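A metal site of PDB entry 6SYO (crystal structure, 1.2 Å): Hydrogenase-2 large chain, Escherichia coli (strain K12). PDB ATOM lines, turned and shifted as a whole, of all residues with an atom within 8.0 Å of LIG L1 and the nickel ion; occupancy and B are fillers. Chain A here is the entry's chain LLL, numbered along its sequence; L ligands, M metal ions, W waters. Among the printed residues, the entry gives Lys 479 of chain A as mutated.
The backbone NH (N) of Ser 502 lies within hydrogen-bond range of a nitrogen (N1) of LG2 L2 (3.1 Å). The side-chain amino group of Lys 479 sits at hydrogen-bond distance from an oxygen (O1) of LIG L1. N of Cys 64 sits close to O2 of LIG L1 (3.4 Å). The backbone NH of Lys 479 lies within hydrogen-bond range of a nitrogen (N2) of LG2 L2, at 3.0 Å. The side-chain hydroxyl (OG) of Ser 502 sits at hydrogen-bond distance from a nitrogen (N1) of LG2 L2 (2.8 Å). SG of Cys 64 binds FE1 of LG2 L2, 2.3 Å away. FE1 of LG2 L2 is bound by SG of Cys 549 (2.3 Å).
O of Cys 64 is in hydrogen-bond range of OG1 of Thr 67 (2.8 Å). OD2 of Asp 544 lies within salt-bridge range of NZ of Lys 479, 2.9 Å away. The side-chain sulfur (SG) of Cys 61 sits close to the backbone NH (N) of Val 63, 3.4 Å away. NZ of Lys 479 is in salt-bridge range of OD1 of Asp 103, at 2.7 Å. The backbone carbonyl oxygen (O) of Val 63 lies close to a ring nitrogen (NE2) of His 99 (3.3 Å). The side-chain hydroxyl of Ser 502 is in hydrogen-bond range of the backbone NH of Cys 546 (3.2 Å). The side-chain sulfur (SG) of Cys 549 sits close to a ring nitrogen (NE2) of His 68 (3.3 Å). SG of Cys 546 sits close to OE1 of Glu 14 (3.5 Å).
Residues that only touch LIG L1: Val 63. Hydrophobic or aromatic side chains within 4 Å of LIG L1: Val 63. Of the 28 residues printed, 5 come within 4 Å of LIG L1. The nearest printed residue that does not touch LIG L1 is Cys 549 (4.02 Å).
The nearest printed residue that does not touch the nickel ion is Val 63 (4.8 Å).
The nickel ion is bound by O2 of LIG L1 (1.9 Å), SG of Cys 546 (2.3 Å), SG of Cys 64 (2.3 Å), SG of Cys 549 (2.3 Å) and SG of Cys 61 (2.4 Å). The nickel ion has five donor atoms within binding distance.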
ATOM      1  N   ILE A  13      -4.315  -2.920  12.540  1.00  0.00           N
ATOM      2  CA  ILE A  13      -3.713  -2.823  13.884  1.00  0.00           C
ATOM      3  C   ILE A  13      -4.792  -3.161  14.899  1.00  0.00           C
ATOM      4  O   ILE A  13      -5.991  -3.326  14.545  1.00  0.00           O
ATOM      5  CB  ILE A  13      -3.149  -1.413  14.176  1.00  0.00           C
ATOM      6  CG1 ILE A  13      -4.281  -0.356  14.238  1.00  0.00           C
ATOM      7  CG2 ILE A  13      -2.027  -0.996  13.178  1.00  0.00           C
ATOM      8  CD1 ILE A  13      -3.788   0.951  14.834  1.00  0.00           C
ATOM      9  N   GLU A  14      -4.451  -3.208  16.178  1.00  0.00           N
ATOM     10  CA  GLU A  14      -5.460  -3.111  17.264  1.00  0.00           C
ATOM     11  C   GLU A  14      -5.689  -1.655  17.625  1.00  0.00           C
ATOM     12  O   GLU A  14      -4.724  -0.909  17.942  1.00  0.00           O
ATOM     13  CB  GLU A  14      -5.042  -3.947  18.495  1.00  0.00           C
ATOM     14  CG  GLU A  14      -6.155  -4.097  19.547  1.00  0.00           C
ATOM     15  CD  GLU A  14      -6.650  -2.829  20.193  1.00  0.00           C
ATOM     16  OE1 GLU A  14      -5.866  -1.917  20.455  1.00  0.00           O
ATOM     17  OE2 GLU A  14      -7.935  -2.707  20.499  1.00  0.00           O
ATOM     18  N   GLN A  58      -7.339  -7.528  32.545  1.00  0.00           N
ATOM     19  CA  GLN A  58      -7.190  -8.366  31.342  1.00  0.00           C
ATOM     20  C   GLN A  58      -7.878  -7.679  30.148  1.00  0.00           C
ATOM     21  O   GLN A  58      -7.392  -7.806  28.994  1.00  0.00           O
ATOM     22  CB  GLN A  58      -7.736  -9.773  31.540  1.00  0.00           C
ATOM     23  CG  GLN A  58      -7.396 -10.694  30.364  1.00  0.00           C
ATOM     24  CD  GLN A  58      -7.642 -12.191  30.503  1.00  0.00           C
ATOM     25  OE1 GLN A  58      -7.049 -12.988  29.724  1.00  0.00           O
ATOM     26  NE2 GLN A  58      -8.597 -12.610  31.370  1.00  0.00           N
ATOM     27  N   ILE A  60      -7.856  -4.674  29.289  1.00  0.00           N
ATOM     28  CA  ILE A  60      -7.085  -3.680  28.550  1.00  0.00           C
ATOM     29  C   ILE A  60      -7.004  -4.088  27.065  1.00  0.00           C
ATOM     30  O   ILE A  60      -7.078  -3.185  26.178  1.00  0.00           O
ATOM     31  CB  ILE A  60      -5.673  -3.463  29.154  1.00  0.00           C
ATOM     32  CG1 ILE A  60      -5.803  -2.682  30.484  1.00  0.00           C
ATOM     33  CG2 ILE A  60      -4.726  -2.771  28.186  1.00  0.00           C
ATOM     34  CD1 ILE A  60      -4.539  -2.593  31.346  1.00  0.00           C
ATOM     35  N   CYS A  61      -6.857  -5.374  26.747  1.00  0.00           N
ATOM     36  CA  CYS A  61      -6.698  -5.801  25.340  1.00  0.00           C
ATOM     37  C   CYS A  61      -7.146  -7.244  25.139  1.00  0.00           C
ATOM     38  O   CYS A  61      -6.745  -8.147  25.902  1.00  0.00           O
ATOM     39  CB  CYS A  61      -5.246  -5.620  24.897  1.00  0.00           C
ATOM     40  SG  CYS A  61      -4.961  -5.884  23.118  1.00  0.00           S
ATOM     41  N   GLY A  62      -7.893  -7.457  24.017  1.00  0.00           N
ATOM     42  CA  GLY A  62      -8.311  -8.788  23.593  1.00  0.00           C
ATOM     43  C   GLY A  62      -7.464  -9.380  22.482  1.00  0.00           C
ATOM     44  O   GLY A  62      -7.684 -10.593  22.182  1.00  0.00           O
ATOM     45  N   VAL A  63      -6.587  -8.604  21.841  1.00  0.00           N
ATOM     46  CA  VAL A  63      -5.594  -9.191  20.907  1.00  0.00           C
ATOM     47  C   VAL A  63      -4.517  -9.841  21.760  1.00  0.00           C
ATOM     48  O   VAL A  63      -4.305 -11.112  21.686  1.00  0.00           O
ATOM     49  CB  VAL A  63      -5.029  -8.187  19.903  1.00  0.00           C
ATOM     50  CG1 VAL A  63      -3.958  -8.875  19.021  1.00  0.00           C
ATOM     51  CG2 VAL A  63      -6.158  -7.625  19.041  1.00  0.00           C
ATOM     52  N   CYS A  64      -3.842  -9.092  22.608  1.00  0.00           N
ATOM     53  CA  CYS A  64      -2.872  -9.644  23.594  1.00  0.00           C
ATOM     54  C   CYS A  64      -3.640 -10.035  24.864  1.00  0.00           C
ATOM     55  O   CYS A  64      -3.234  -9.726  26.017  1.00  0.00           O
ATOM     56  CB  CYS A  64      -1.685  -8.709  23.800  1.00  0.00           C
ATOM     57  SG  CYS A  64      -2.058  -7.120  24.566  1.00  0.00           S
ATOM     58  N   THR A  65      -4.706 -10.801  24.701  1.00  0.00           N
ATOM     59  CA  THR A  65      -5.405 -11.487  25.828  1.00  0.00           C
ATOM     60  C   THR A  65      -4.357 -12.372  26.562  1.00  0.00           C
ATOM     61  O   THR A  65      -3.263 -12.678  25.979  1.00  0.00           O
ATOM     62  CB  THR A  65      -6.696 -12.183  25.366  1.00  0.00           C
ATOM     63  OG1 THR A  65      -7.408 -12.615  26.534  1.00  0.00           O
ATOM     64  CG2 THR A  65      -6.411 -13.400  24.482  1.00  0.00           C
ATOM     65  N   THR A  67      -2.106 -11.554  28.654  1.00  0.00           N
ATOM     66  CA  THR A  67      -0.851 -10.917  29.064  1.00  0.00           C
ATOM     67  C   THR A  67      -1.097  -9.999  30.302  1.00  0.00           C
ATOM     68  O   THR A  67      -0.290 -10.025  31.268  1.00  0.00           O
ATOM     69  CB  THR A  67      -0.227 -10.090  27.918  1.00  0.00           C
ATOM     70  OG1 THR A  67      -0.973  -8.957  27.536  1.00  0.00           O
ATOM     71  CG2 THR A  67       0.160 -10.984  26.744  1.00  0.00           C
ATOM     72  N   HIS A  68      -2.124  -9.179  30.272  1.00  0.00           N
ATOM     73  CA  HIS A  68      -2.407  -8.251  31.388  1.00  0.00           C
ATOM     74  C   HIS A  68      -2.926  -9.031  32.608  1.00  0.00           C
ATOM     75  O   HIS A  68      -2.701  -8.592  33.759  1.00  0.00           O
ATOM     76  CB  HIS A  68      -3.397  -7.151  30.938  1.00  0.00           C
ATOM     77  CG  HIS A  68      -2.843  -6.227  29.925  1.00  0.00           C
ATOM     78  ND1 HIS A  68      -1.906  -5.231  30.249  1.00  0.00           N
ATOM     79  CD2 HIS A  68      -3.013  -6.207  28.568  1.00  0.00           C
ATOM     80  CE1 HIS A  68      -1.561  -4.653  29.100  1.00  0.00           C
ATOM     81  NE2 HIS A  68      -2.230  -5.200  28.038  1.00  0.00           N
ATOM     82  N   HIS A  99      -0.513 -18.702  23.286  1.00  0.00           N
ATOM     83  CA  HIS A  99      -1.151 -17.402  22.891  1.00  0.00           C
ATOM     84  C   HIS A  99      -0.243 -16.605  21.943  1.00  0.00           C
ATOM     85  O   HIS A  99      -0.671 -16.103  20.881  1.00  0.00           O
ATOM     86  CB  HIS A  99      -1.491 -16.528  24.133  1.00  0.00           C
ATOM     87  CG  HIS A  99      -1.918 -15.171  23.627  1.00  0.00           C
ATOM     88  ND1 HIS A  99      -3.183 -14.980  23.135  1.00  0.00           N
ATOM     89  CD2 HIS A  99      -1.187 -14.069  23.350  1.00  0.00           C
ATOM     90  CE1 HIS A  99      -3.183 -13.746  22.608  1.00  0.00           C
ATOM     91  NE2 HIS A  99      -1.941 -13.173  22.636  1.00  0.00           N
ATOM     92  N   ASP A 103      -0.692 -15.030  18.174  1.00  0.00           N
ATOM     93  CA  ASP A 103      -0.580 -13.571  17.988  1.00  0.00           C
ATOM     94  C   ASP A 103       0.393 -13.241  16.811  1.00  0.00           C
ATOM     95  O   ASP A 103       0.076 -12.439  15.912  1.00  0.00           O
ATOM     96  CB  ASP A 103      -0.113 -13.001  19.337  1.00  0.00           C
ATOM     97  CG  ASP A 103      -0.377 -11.605  19.660  1.00  0.00           C
ATOM     98  OD1 ASP A 103       0.081 -10.805  18.758  1.00  0.00           O
ATOM     99  OD2 ASP A 103      -0.833 -11.233  20.789  1.00  0.00           O
ATOM    100  N   HIS A 107      -0.430 -11.584  13.113  1.00  0.00           N
ATOM    101  CA  HIS A 107       0.201 -10.298  12.747  1.00  0.00           C
ATOM    102  C   HIS A 107       0.878 -10.396  11.352  1.00  0.00           C
ATOM    103  O   HIS A 107       0.696  -9.470  10.487  1.00  0.00           O
ATOM    104  CB  HIS A 107       1.222  -9.787  13.777  1.00  0.00           C
ATOM    105  CG  HIS A 107       1.743  -8.443  13.380  1.00  0.00           C
ATOM    106  ND1 HIS A 107       3.037  -8.287  12.803  1.00  0.00           N
ATOM    107  CD2 HIS A 107       1.104  -7.239  13.321  1.00  0.00           C
ATOM    108  CE1 HIS A 107       3.147  -6.986  12.483  1.00  0.00           C
ATOM    109  NE2 HIS A 107       1.971  -6.308  12.759  1.00  0.00           N
ATOM    110  N   LEU A 111      -2.635  -9.070   9.403  1.00  0.00           N
ATOM    111  CA  LEU A 111      -2.423  -7.629   9.632  1.00  0.00           C
ATOM    112  C   LEU A 111      -1.364  -7.088   8.660  1.00  0.00           C
ATOM    113  O   LEU A 111      -1.591  -6.000   8.092  1.00  0.00           O
ATOM    114  CB  LEU A 111      -2.125  -7.329  11.100  1.00  0.00           C
ATOM    115  CG  LEU A 111      -3.111  -7.897  12.134  1.00  0.00           C
ATOM    116  CD1 LEU A 111      -2.751  -7.475  13.541  1.00  0.00           C
ATOM    117  CD2 LEU A 111      -4.527  -7.471  11.835  1.00  0.00           C
ATOM    118  N   ALA A 477       5.747  -9.764  26.739  1.00  0.00           N
ATOM    119  CA  ALA A 477       4.525  -9.933  25.940  1.00  0.00           C
ATOM    120  C   ALA A 477       4.885 -10.020  24.459  1.00  0.00           C
ATOM    121  O   ALA A 477       6.004  -9.712  24.013  1.00  0.00           O
ATOM    122  CB  ALA A 477       3.567  -8.767  26.230  1.00  0.00           C
ATOM    123  N   PRO A 478       3.897 -10.384  23.586  1.00  0.00           N
ATOM    124  CA  PRO A 478       4.172 -10.437  22.154  1.00  0.00           C
ATOM    125  C   PRO A 478       4.726  -9.130  21.544  1.00  0.00           C
ATOM    126  O   PRO A 478       5.526  -9.190  20.559  1.00  0.00           O
ATOM    127  CB  PRO A 478       2.798 -10.864  21.531  1.00  0.00           C
ATOM    128  CG  PRO A 478       2.140 -11.677  22.642  1.00  0.00           C
ATOM    129  CD  PRO A 478       2.544 -10.924  23.901  1.00  0.00           C
ATOM    130  N   LYS A 479       4.289  -7.966  22.051  1.00  0.00           N
ATOM    131  CA  LYS A 479       4.751  -6.651  21.596  1.00  0.00           C
ATOM    132  C   LYS A 479       5.946  -6.118  22.424  1.00  0.00           C
ATOM    133  O   LYS A 479       6.460  -5.047  22.060  1.00  0.00           O
ATOM    134  CB  LYS A 479       3.611  -5.618  21.584  1.00  0.00           C
ATOM    135  CG  LYS A 479       2.832  -5.483  20.287  1.00  0.00           C
ATOM    136  CD  LYS A 479       1.444  -6.121  20.198  1.00  0.00           C
ATOM    137  CE  LYS A 479       1.439  -7.627  20.112  1.00  0.00           C
ATOM    138  NZ  LYS A 479       0.298  -8.121  19.228  1.00  0.00           N
ATOM    139  N   VAL A 500       2.971  -0.258  29.184  1.00  0.00           N
ATOM    140  CA  VAL A 500       2.673  -1.351  28.255  1.00  0.00           C
ATOM    141  C   VAL A 500       3.625  -1.255  27.059  1.00  0.00           C
ATOM    142  O   VAL A 500       4.116  -0.148  26.746  1.00  0.00           O
ATOM    143  CB  VAL A 500       1.168  -1.271  27.886  1.00  0.00           C
ATOM    144  CG1 VAL A 500       0.681  -2.449  27.073  1.00  0.00           C
ATOM    145  CG2 VAL A 500       0.315  -1.204  29.171  1.00  0.00           C
ATOM    146  N   PRO A 501       4.009  -2.359  26.366  1.00  0.00           N
ATOM    147  CA  PRO A 501       5.046  -2.237  25.317  1.00  0.00           C
ATOM    148  C   PRO A 501       4.713  -1.217  24.224  1.00  0.00           C
ATOM    149  O   PRO A 501       5.588  -0.396  23.850  1.00  0.00           O
ATOM    150  CB  PRO A 501       5.248  -3.671  24.768  1.00  0.00           C
ATOM    151  CG  PRO A 501       4.103  -4.463  25.347  1.00  0.00           C
ATOM    152  CD  PRO A 501       3.715  -3.779  26.669  1.00  0.00           C
ATOM    153  N   SER A 502       3.460  -1.166  23.733  1.00  0.00           N
ATOM    154  CA  SER A 502       3.125  -0.129  22.707  1.00  0.00           C
ATOM    155  C   SER A 502       3.193   1.270  23.304  1.00  0.00           C
ATOM    156  O   SER A 502       3.307   2.264  22.525  1.00  0.00           O
ATOM    157  CB  SER A 502       1.789  -0.415  21.994  1.00  0.00           C
ATOM    158  OG  SER A 502       1.848  -1.576  21.172  1.00  0.00           O
ATOM    159  N   ASP A 544       3.846  -3.711  15.170  1.00  0.00           N
ATOM    160  CA  ASP A 544       2.620  -4.388  15.670  1.00  0.00           C
ATOM    161  C   ASP A 544       1.881  -3.487  16.676  1.00  0.00           C
ATOM    162  O   ASP A 544       1.631  -3.846  17.857  1.00  0.00           O
ATOM    163  CB  ASP A 544       3.021  -5.752  16.244  1.00  0.00           C
ATOM    164  CG  ASP A 544       1.941  -6.728  16.615  1.00  0.00           C
ATOM    165  OD1 ASP A 544       0.753  -6.522  16.313  1.00  0.00           O
ATOM    166  OD2 ASP A 544       2.369  -7.786  17.201  1.00  0.00           O
ATOM    167  N   PRO A 545       1.405  -2.308  16.222  1.00  0.00           N
ATOM    168  CA  PRO A 545       0.705  -1.393  17.144  1.00  0.00           C
ATOM    169  C   PRO A 545      -0.539  -2.002  17.814  1.00  0.00           C
ATOM    170  O   PRO A 545      -1.391  -2.637  17.209  1.00  0.00           O
ATOM    171  CB  PRO A 545       0.305  -0.200  16.294  1.00  0.00           C
ATOM    172  CG  PRO A 545       1.276  -0.247  15.106  1.00  0.00           C
ATOM    173  CD  PRO A 545       1.485  -1.725  14.854  1.00  0.00           C
ATOM    174  N   CYS A 546      -0.659  -1.706  19.133  1.00  0.00           N
ATOM    175  CA  CYS A 546      -1.815  -2.068  19.934  1.00  0.00           C
ATOM    176  C   CYS A 546      -2.224  -0.809  20.781  1.00  0.00           C
ATOM    177  O   CYS A 546      -1.521  -0.500  21.779  1.00  0.00           O
ATOM    178  CB  CYS A 546      -1.577  -3.285  20.803  1.00  0.00           C
ATOM    179  SG  CYS A 546      -3.106  -3.765  21.679  1.00  0.00           S
ATOM    180  N   MET A 547      -3.267  -0.072  20.346  1.00  0.00           N
ATOM    181  CA  MET A 547      -3.539   1.231  21.000  1.00  0.00           C
ATOM    182  C   MET A 547      -4.435   1.073  22.228  1.00  0.00           C
ATOM    183  O   MET A 547      -4.375   1.979  23.149  1.00  0.00           O
ATOM    184  CB  MET A 547      -4.148   2.237  20.005  1.00  0.00           C
ATOM    185  CG  MET A 547      -3.222   2.439  18.755  1.00  0.00           C
ATOM    186  SD  MET A 547      -1.440   2.673  19.091  1.00  0.00           S
ATOM    187  CE  MET A 547      -1.526   4.229  19.939  1.00  0.00           C
ATOM    188  N   ALA A 548      -5.253   0.031  22.333  1.00  0.00           N
ATOM    189  CA  ALA A 548      -5.944  -0.310  23.610  1.00  0.00           C
ATOM    190  C   ALA A 548      -4.877  -0.573  24.680  1.00  0.00           C
ATOM    191  O   ALA A 548      -4.936  -0.034  25.837  1.00  0.00           O
ATOM    192  CB  ALA A 548      -6.899  -1.488  23.418  1.00  0.00           C
ATOM    193  N   CYS A 549      -3.855  -1.334  24.327  1.00  0.00           N
ATOM    194  CA  CYS A 549      -2.649  -1.511  25.187  1.00  0.00           C
ATOM    195  C   CYS A 549      -1.943  -0.186  25.450  1.00  0.00           C
ATOM    196  O   CYS A 549      -1.587   0.095  26.622  1.00  0.00           O
ATOM    197  CB  CYS A 549      -1.708  -2.529  24.506  1.00  0.00           C
ATOM    198  SG  CYS A 549      -2.074  -4.226  24.895  1.00  0.00           S
ATOM    199  N   ALA A 550      -1.616   0.592  24.394  1.00  0.00           N
ATOM    200  CA  ALA A 550      -0.752   1.776  24.611  1.00  0.00           C
ATOM    201  C   ALA A 550      -1.381   2.747  25.606  1.00  0.00           C
ATOM    202  O   ALA A 550      -0.659   3.381  26.380  1.00  0.00           O
ATOM    203  CB  ALA A 550      -0.500   2.469  23.291  1.00  0.00           C
HETATM  204  O1  LIG L   1      -1.790  -6.924  20.451  1.00  0.00           O
HETATM  205  O2  LIG L   1      -2.014  -6.412  21.519  1.00  0.00           O
HETATM  206 FE1  LG2 L   2      -0.346  -5.650  24.368  1.00  0.00          FE
HETATM  207  C1  LG2 L   2       0.678  -4.277  23.681  1.00  0.00           C
HETATM  208  N1  LG2 L   2       1.369  -3.375  23.285  1.00  0.00           N
HETATM  209  C2  LG2 L   2       0.876  -6.938  23.725  1.00  0.00           C
HETATM  210  N2  LG2 L   2       1.621  -7.793  23.410  1.00  0.00           N
HETATM  211  C3  LG2 L   2       0.491  -5.820  25.911  1.00  0.00           C
HETATM  212  O1  LG2 L   2       1.094  -5.941  26.902  1.00  0.00           O
HETATM  213 NI    NI M   1      -2.617  -5.504  23.031  1.00  0.00          NI
HETATM  214  O   HOH W   1      -2.325  -5.842  17.831  1.00  0.00           O
